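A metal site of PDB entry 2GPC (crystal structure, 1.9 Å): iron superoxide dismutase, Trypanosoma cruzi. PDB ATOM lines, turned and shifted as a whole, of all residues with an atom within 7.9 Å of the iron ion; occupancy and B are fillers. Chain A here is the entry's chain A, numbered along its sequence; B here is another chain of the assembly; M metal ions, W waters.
Water W1 lies within hydrogen-bond range of the side-chain carboxylate of Asp 160 and the side-chain amide nitrogen of Gln 71.
The iron ion is bound by OD2 of Asp 160 (2.0 Å), NE2 of His 164 (2.1 Å), NE2 of His 75 (2.1 Å), NE2 of His 27 (2.1 Å) and water W1 (2.3 Å).
The iron ion has five donor atoms within binding distance.
Four residues have an atom within 4 Å of the iron ion: His 27, His 75, Asp 160 and His 164.
Along chain A the residues within 4 Å of the iron ion span positions 27 to 164.
The nearest printed residue that does not touch the iron ion is Trp 124 (4.4 Å).
The backbone NH (N) of Trp 162 is in hydrogen-bond range of the side-chain carboxylate (OD1) of Asp 160, at 3.0 Å.
The side-chain hydroxyl of Tyr 177 sits at hydrogen-bond distance from the backbone carbonyl oxygen of Asp 160, 2.6 Å away.
O of His 27 is in hydrogen-bond range of N of His 32, at 3.0 Å.
A ring nitrogen (ND1) of His 164 sits at hydrogen-bond distance from the side-chain carboxylate of Glu 163 of chain B.
The backbone carbonyl oxygen of His 75 sits close to the indole nitrogen of Trp 79 (3.4 Å).
The backbone carbonyl oxygen (O) of Gln 71 sits at hydrogen-bond distance from a ring nitrogen (ND1) of His 75, 2.6 Å away.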
ATOM      1  N   HIS A  27      23.872  28.212 -23.119  1.00  0.00           N
ATOM      2  CA  HIS A  27      23.188  26.926 -23.240  1.00  0.00           C
ATOM      3  C   HIS A  27      23.207  26.417 -24.709  1.00  0.00           C
ATOM      4  O   HIS A  27      23.500  25.249 -24.954  1.00  0.00           O
ATOM      5  CB  HIS A  27      21.768  27.042 -22.658  1.00  0.00           C
ATOM      6  CG  HIS A  27      21.112  25.734 -22.337  1.00  0.00           C
ATOM      7  ND1 HIS A  27      19.818  25.658 -21.891  1.00  0.00           N
ATOM      8  CD2 HIS A  27      21.583  24.456 -22.376  1.00  0.00           C
ATOM      9  CE1 HIS A  27      19.506  24.387 -21.669  1.00  0.00           C
ATOM     10  NE2 HIS A  27      20.556  23.642 -21.959  1.00  0.00           N
ATOM     11  N   TYR A  28      22.988  27.303 -25.680  1.00  0.00           N
ATOM     12  CA  TYR A  28      22.941  26.924 -27.091  1.00  0.00           C
ATOM     13  C   TYR A  28      24.330  26.799 -27.712  1.00  0.00           C
ATOM     14  O   TYR A  28      24.649  25.783 -28.314  1.00  0.00           O
ATOM     15  CB  TYR A  28      22.083  27.931 -27.895  1.00  0.00           C
ATOM     16  CG  TYR A  28      21.881  27.545 -29.342  1.00  0.00           C
ATOM     17  CD1 TYR A  28      20.833  26.696 -29.719  1.00  0.00           C
ATOM     18  CD2 TYR A  28      22.746  27.996 -30.337  1.00  0.00           C
ATOM     19  CE1 TYR A  28      20.641  26.328 -31.039  1.00  0.00           C
ATOM     20  CE2 TYR A  28      22.566  27.631 -31.677  1.00  0.00           C
ATOM     21  CZ  TYR A  28      21.515  26.784 -32.023  1.00  0.00           C
ATOM     22  OH  TYR A  28      21.312  26.408 -33.341  1.00  0.00           O
ATOM     23  N   HIS A  31      26.775  24.366 -24.780  1.00  0.00           N
ATOM     24  CA  HIS A  31      26.276  23.020 -24.494  1.00  0.00           C
ATOM     25  C   HIS A  31      25.702  22.356 -25.740  1.00  0.00           C
ATOM     26  O   HIS A  31      26.184  21.304 -26.136  1.00  0.00           O
ATOM     27  CB  HIS A  31      25.272  23.011 -23.320  1.00  0.00           C
ATOM     28  CG  HIS A  31      25.885  23.418 -22.029  1.00  0.00           C
ATOM     29  ND1 HIS A  31      26.618  22.546 -21.246  1.00  0.00           N
ATOM     30  CD2 HIS A  31      25.933  24.616 -21.385  1.00  0.00           C
ATOM     31  CE1 HIS A  31      27.085  23.184 -20.188  1.00  0.00           C
ATOM     32  NE2 HIS A  31      26.685  24.437 -20.252  1.00  0.00           N
ATOM     33  N   HIS A  32      24.720  22.968 -26.380  1.00  0.00           N
ATOM     34  CA  HIS A  32      24.018  22.312 -27.481  1.00  0.00           C
ATOM     35  C   HIS A  32      24.938  22.116 -28.685  1.00  0.00           C
ATOM     36  O   HIS A  32      25.057  20.999 -29.201  1.00  0.00           O
ATOM     37  CB  HIS A  32      22.762  23.089 -27.874  1.00  0.00           C
ATOM     38  CG  HIS A  32      21.760  22.285 -28.648  1.00  0.00           C
ATOM     39  ND1 HIS A  32      20.620  22.848 -29.171  1.00  0.00           N
ATOM     40  CD2 HIS A  32      21.724  20.974 -28.990  1.00  0.00           C
ATOM     41  CE1 HIS A  32      19.914  21.922 -29.799  1.00  0.00           C
ATOM     42  NE2 HIS A  32      20.577  20.770 -29.701  1.00  0.00           N
ATOM     43  N   TYR A  35      27.694  19.461 -28.150  1.00  0.00           N
ATOM     44  CA  TYR A  35      27.282  18.087 -28.414  1.00  0.00           C
ATOM     45  C   TYR A  35      27.371  17.773 -29.904  1.00  0.00           C
ATOM     46  O   TYR A  35      27.791  16.686 -30.292  1.00  0.00           O
ATOM     47  CB  TYR A  35      25.852  17.837 -27.903  1.00  0.00           C
ATOM     48  CG  TYR A  35      25.710  17.850 -26.402  1.00  0.00           C
ATOM     49  CD1 TYR A  35      26.498  17.020 -25.603  1.00  0.00           C
ATOM     50  CD2 TYR A  35      24.791  18.681 -25.768  1.00  0.00           C
ATOM     51  CE1 TYR A  35      26.367  17.008 -24.234  1.00  0.00           C
ATOM     52  CE2 TYR A  35      24.653  18.675 -24.375  1.00  0.00           C
ATOM     53  CZ  TYR A  35      25.444  17.825 -23.619  1.00  0.00           C
ATOM     54  OH  TYR A  35      25.351  17.805 -22.266  1.00  0.00           O
ATOM     55  N   GLN A  71      21.230  14.184 -26.404  1.00  0.00           N
ATOM     56  CA  GLN A  71      21.282  15.555 -25.900  1.00  0.00           C
ATOM     57  C   GLN A  71      20.983  16.545 -27.010  1.00  0.00           C
ATOM     58  O   GLN A  71      20.368  17.570 -26.772  1.00  0.00           O
ATOM     59  CB  GLN A  71      22.636  15.869 -25.247  1.00  0.00           C
ATOM     60  CG  GLN A  71      22.821  15.243 -23.861  1.00  0.00           C
ATOM     61  CD  GLN A  71      21.908  15.831 -22.812  1.00  0.00           C
ATOM     62  OE1 GLN A  71      20.746  15.449 -22.727  1.00  0.00           O
ATOM     63  NE2 GLN A  71      22.417  16.772 -22.014  1.00  0.00           N
ATOM     64  N   ASN A  74      17.154  16.270 -27.488  1.00  0.00           N
ATOM     65  CA  ASN A  74      16.424  16.812 -26.320  1.00  0.00           C
ATOM     66  C   ASN A  74      16.491  18.349 -26.291  1.00  0.00           C
ATOM     67  O   ASN A  74      15.505  18.995 -25.985  1.00  0.00           O
ATOM     68  CB  ASN A  74      16.977  16.255 -24.990  1.00  0.00           C
ATOM     69  CG  ASN A  74      16.745  14.759 -24.826  1.00  0.00           C
ATOM     70  OD1 ASN A  74      15.913  14.180 -25.493  1.00  0.00           O
ATOM     71  ND2 ASN A  74      17.507  14.134 -23.910  1.00  0.00           N
ATOM     72  N   HIS A  75      17.649  18.908 -26.644  1.00  0.00           N
ATOM     73  CA  HIS A  75      17.827  20.364 -26.605  1.00  0.00           C
ATOM     74  C   HIS A  75      16.994  21.032 -27.691  1.00  0.00           C
ATOM     75  O   HIS A  75      16.333  22.025 -27.442  1.00  0.00           O
ATOM     76  CB  HIS A  75      19.307  20.763 -26.704  1.00  0.00           C
ATOM     77  CG  HIS A  75      20.025  20.640 -25.406  1.00  0.00           C
ATOM     78  ND1 HIS A  75      20.474  19.424 -24.931  1.00  0.00           N
ATOM     79  CD2 HIS A  75      20.300  21.546 -24.446  1.00  0.00           C
ATOM     80  CE1 HIS A  75      21.014  19.599 -23.735  1.00  0.00           C
ATOM     81  NE2 HIS A  75      20.937  20.873 -23.421  1.00  0.00           N
ATOM     82  N   TYR A  78      13.525  21.035 -26.625  1.00  0.00           N
ATOM     83  CA  TYR A  78      13.408  21.998 -25.527  1.00  0.00           C
ATOM     84  C   TYR A  78      13.187  23.432 -26.034  1.00  0.00           C
ATOM     85  O   TYR A  78      12.292  24.137 -25.548  1.00  0.00           O
ATOM     86  CB  TYR A  78      14.658  21.904 -24.664  1.00  0.00           C
ATOM     87  CG  TYR A  78      14.840  22.974 -23.620  1.00  0.00           C
ATOM     88  CD1 TYR A  78      13.914  23.168 -22.590  1.00  0.00           C
ATOM     89  CD2 TYR A  78      15.980  23.763 -23.614  1.00  0.00           C
ATOM     90  CE1 TYR A  78      14.120  24.135 -21.599  1.00  0.00           C
ATOM     91  CE2 TYR A  78      16.191  24.737 -22.649  1.00  0.00           C
ATOM     92  CZ  TYR A  78      15.262  24.916 -21.640  1.00  0.00           C
ATOM     93  OH  TYR A  78      15.497  25.887 -20.693  1.00  0.00           O
ATOM     94  N   TRP A  79      13.984  23.871 -27.017  1.00  0.00           N
ATOM     95  CA  TRP A  79      13.790  25.205 -27.591  1.00  0.00           C
ATOM     96  C   TRP A  79      12.437  25.315 -28.292  1.00  0.00           C
ATOM     97  O   TRP A  79      11.770  26.360 -28.210  1.00  0.00           O
ATOM     98  CB  TRP A  79      14.909  25.581 -28.587  1.00  0.00           C
ATOM     99  CG  TRP A  79      16.309  25.362 -28.106  1.00  0.00           C
ATOM    100  CD1 TRP A  79      17.277  24.631 -28.725  1.00  0.00           C
ATOM    101  CD2 TRP A  79      16.923  25.938 -26.942  1.00  0.00           C
ATOM    102  NE1 TRP A  79      18.446  24.690 -28.011  1.00  0.00           N
ATOM    103  CE2 TRP A  79      18.258  25.489 -26.914  1.00  0.00           C
ATOM    104  CE3 TRP A  79      16.485  26.782 -25.919  1.00  0.00           C
ATOM    105  CZ2 TRP A  79      19.149  25.841 -25.898  1.00  0.00           C
ATOM    106  CZ3 TRP A  79      17.367  27.130 -24.913  1.00  0.00           C
ATOM    107  CH2 TRP A  79      18.682  26.663 -24.910  1.00  0.00           C
ATOM    108  N   GLY A 123      18.812  16.085 -15.573  1.00  0.00           N
ATOM    109  CA  GLY A 123      17.704  15.426 -16.226  1.00  0.00           C
ATOM    110  C   GLY A 123      16.748  16.322 -16.992  1.00  0.00           C
ATOM    111  O   GLY A 123      17.052  17.464 -17.288  1.00  0.00           O
ATOM    112  N   TRP A 124      15.587  15.756 -17.280  1.00  0.00           N
ATOM    113  CA  TRP A 124      14.593  16.301 -18.225  1.00  0.00           C
ATOM    114  C   TRP A 124      13.200  15.916 -17.727  1.00  0.00           C
ATOM    115  O   TRP A 124      12.962  14.762 -17.375  1.00  0.00           O
ATOM    116  CB  TRP A 124      14.783  15.686 -19.616  1.00  0.00           C
ATOM    117  CG  TRP A 124      16.086  15.962 -20.283  1.00  0.00           C
ATOM    118  CD1 TRP A 124      17.214  15.218 -20.217  1.00  0.00           C
ATOM    119  CD2 TRP A 124      16.383  17.076 -21.121  1.00  0.00           C
ATOM    120  NE1 TRP A 124      18.211  15.809 -20.957  1.00  0.00           N
ATOM    121  CE2 TRP A 124      17.724  16.948 -21.521  1.00  0.00           C
ATOM    122  CE3 TRP A 124      15.642  18.174 -21.581  1.00  0.00           C
ATOM    123  CZ2 TRP A 124      18.351  17.876 -22.358  1.00  0.00           C
ATOM    124  CZ3 TRP A 124      16.266  19.093 -22.420  1.00  0.00           C
ATOM    125  CH2 TRP A 124      17.615  18.939 -22.789  1.00  0.00           C
ATOM    126  N   ASP A 160      14.350  21.183 -19.680  1.00  0.00           N
ATOM    127  CA  ASP A 160      15.687  20.819 -19.262  1.00  0.00           C
ATOM    128  C   ASP A 160      15.877  21.233 -17.817  1.00  0.00           C
ATOM    129  O   ASP A 160      15.673  22.393 -17.487  1.00  0.00           O
ATOM    130  CB  ASP A 160      16.694  21.579 -20.134  1.00  0.00           C
ATOM    131  CG  ASP A 160      18.124  21.113 -19.976  1.00  0.00           C
ATOM    132  OD1 ASP A 160      18.428  20.185 -19.170  1.00  0.00           O
ATOM    133  OD2 ASP A 160      19.032  21.633 -20.673  1.00  0.00           O
ATOM    134  N   VAL A 161      16.247  20.293 -16.954  1.00  0.00           N
ATOM    135  CA  VAL A 161      16.557  20.631 -15.555  1.00  0.00           C
ATOM    136  C   VAL A 161      18.001  20.293 -15.166  1.00  0.00           C
ATOM    137  O   VAL A 161      18.337  20.278 -13.977  1.00  0.00           O
ATOM    138  CB  VAL A 161      15.527  20.033 -14.540  1.00  0.00           C
ATOM    139  CG1 VAL A 161      14.134  20.599 -14.797  1.00  0.00           C
ATOM    140  CG2 VAL A 161      15.514  18.502 -14.547  1.00  0.00           C
ATOM    141  N   TRP A 162      18.868  20.078 -16.169  1.00  0.00           N
ATOM    142  CA  TRP A 162      20.306  20.173 -15.940  1.00  0.00           C
ATOM    143  C   TRP A 162      20.557  21.557 -15.372  1.00  0.00           C
ATOM    144  O   TRP A 162      19.933  22.534 -15.809  1.00  0.00           O
ATOM    145  CB  TRP A 162      21.107  20.000 -17.239  1.00  0.00           C
ATOM    146  CG  TRP A 162      21.244  18.581 -17.752  1.00  0.00           C
ATOM    147  CD1 TRP A 162      20.241  17.734 -18.118  1.00  0.00           C
ATOM    148  CD2 TRP A 162      22.469  17.877 -17.998  1.00  0.00           C
ATOM    149  NE1 TRP A 162      20.762  16.541 -18.572  1.00  0.00           N
ATOM    150  CE2 TRP A 162      22.124  16.598 -18.505  1.00  0.00           C
ATOM    151  CE3 TRP A 162      23.823  18.191 -17.848  1.00  0.00           C
ATOM    152  CZ2 TRP A 162      23.080  15.638 -18.852  1.00  0.00           C
ATOM    153  CZ3 TRP A 162      24.770  17.251 -18.176  1.00  0.00           C
ATOM    154  CH2 TRP A 162      24.397  15.979 -18.673  1.00  0.00           C
ATOM    155  N   GLU A 163      21.434  21.653 -14.384  1.00  0.00           N
ATOM    156  CA  GLU A 163      21.748  22.914 -13.730  1.00  0.00           C
ATOM    157  C   GLU A 163      22.212  24.008 -14.693  1.00  0.00           C
ATOM    158  O   GLU A 163      21.881  25.169 -14.482  1.00  0.00           O
ATOM    159  CB  GLU A 163      22.771  22.686 -12.595  1.00  0.00           C
ATOM    160  CG  GLU A 163      22.148  21.897 -11.458  1.00  0.00           C
ATOM    161  CD  GLU A 163      23.087  21.623 -10.294  1.00  0.00           C
ATOM    162  OE1 GLU A 163      24.279  21.313 -10.530  1.00  0.00           O
ATOM    163  OE2 GLU A 163      22.601  21.681  -9.142  1.00  0.00           O
ATOM    164  N   HIS A 164      22.923  23.629 -15.761  1.00  0.00           N
ATOM    165  CA  HIS A 164      23.372  24.587 -16.772  1.00  0.00           C
ATOM    166  C   HIS A 164      22.215  25.290 -17.508  1.00  0.00           C
ATOM    167  O   HIS A 164      22.405  26.348 -18.077  1.00  0.00           O
ATOM    168  CB  HIS A 164      24.331  23.933 -17.784  1.00  0.00           C
ATOM    169  CG  HIS A 164      23.692  22.943 -18.714  1.00  0.00           C
ATOM    170  ND1 HIS A 164      24.165  21.660 -18.867  1.00  0.00           N
ATOM    171  CD2 HIS A 164      22.645  23.060 -19.577  1.00  0.00           C
ATOM    172  CE1 HIS A 164      23.440  21.020 -19.766  1.00  0.00           C
ATOM    173  NE2 HIS A 164      22.513  21.847 -20.215  1.00  0.00           N
ATOM    174  N   ALA A 165      21.037  24.690 -17.494  1.00  0.00           N
ATOM    175  CA  ALA A 165      19.870  25.285 -18.141  1.00  0.00           C
ATOM    176  C   ALA A 165      19.377  26.555 -17.427  1.00  0.00           C
ATOM    177  O   ALA A 165      18.757  27.425 -18.042  1.00  0.00           O
ATOM    178  CB  ALA A 165      18.751  24.266 -18.250  1.00  0.00           C
ATOM    179  N   TYR A 166      19.663  26.667 -16.125  1.00  0.00           N
ATOM    180  CA  TYR A 166      19.108  27.744 -15.312  1.00  0.00           C
ATOM    181  C   TYR A 166      20.076  28.442 -14.365  1.00  0.00           C
ATOM    182  O   TYR A 166      19.712  29.457 -13.773  1.00  0.00           O
ATOM    183  CB  TYR A 166      17.911  27.214 -14.495  1.00  0.00           C
ATOM    184  CG  TYR A 166      18.204  26.089 -13.506  1.00  0.00           C
ATOM    185  CD1 TYR A 166      18.679  26.349 -12.226  1.00  0.00           C
ATOM    186  CD2 TYR A 166      17.987  24.765 -13.870  1.00  0.00           C
ATOM    187  CE1 TYR A 166      18.929  25.318 -11.326  1.00  0.00           C
ATOM    188  CE2 TYR A 166      18.236  23.734 -12.969  1.00  0.00           C
ATOM    189  CZ  TYR A 166      18.704  24.007 -11.718  1.00  0.00           C
ATOM    190  OH  TYR A 166      18.927  22.976 -10.853  1.00  0.00           O
ATOM    191  N   TYR A 177      12.879  28.866 -11.825  1.00  0.00           N
ATOM    192  CA  TYR A 177      13.120  28.601 -13.238  1.00  0.00           C
ATOM    193  C   TYR A 177      11.936  27.860 -13.863  1.00  0.00           C
ATOM    194  O   TYR A 177      11.539  28.166 -14.979  1.00  0.00           O
ATOM    195  CB  TYR A 177      14.412  27.770 -13.391  1.00  0.00           C
ATOM    196  CG  TYR A 177      14.529  26.990 -14.687  1.00  0.00           C
ATOM    197  CD1 TYR A 177      14.659  27.633 -15.922  1.00  0.00           C
ATOM    198  CD2 TYR A 177      14.533  25.593 -14.676  1.00  0.00           C
ATOM    199  CE1 TYR A 177      14.772  26.908 -17.114  1.00  0.00           C
ATOM    200  CE2 TYR A 177      14.643  24.865 -15.854  1.00  0.00           C
ATOM    201  CZ  TYR A 177      14.761  25.518 -17.074  1.00  0.00           C
ATOM    202  OH  TYR A 177      14.897  24.779 -18.250  1.00  0.00           O
ATOM    203  N   GLU B 163      27.361  20.548 -11.890  1.00  0.00           N
ATOM    204  CA  GLU B 163      27.540  21.827 -12.559  1.00  0.00           C
ATOM    205  C   GLU B 163      27.481  23.035 -11.606  1.00  0.00           C
ATOM    206  O   GLU B 163      28.161  24.022 -11.845  1.00  0.00           O
ATOM    207  CB  GLU B 163      26.544  21.967 -13.727  1.00  0.00           C
ATOM    208  CG  GLU B 163      26.836  20.991 -14.857  1.00  0.00           C
ATOM    209  CD  GLU B 163      25.850  21.086 -16.005  1.00  0.00           C
ATOM    210  OE1 GLU B 163      24.649  21.219 -15.737  1.00  0.00           O
ATOM    211  OE2 GLU B 163      26.295  21.017 -17.176  1.00  0.00           O
HETATM  212 FE    FE M   1      20.858  21.586 -21.445  1.00  0.00          FE
HETATM  213  O   HOH W   1      20.802  19.430 -20.739  1.00  0.00           O
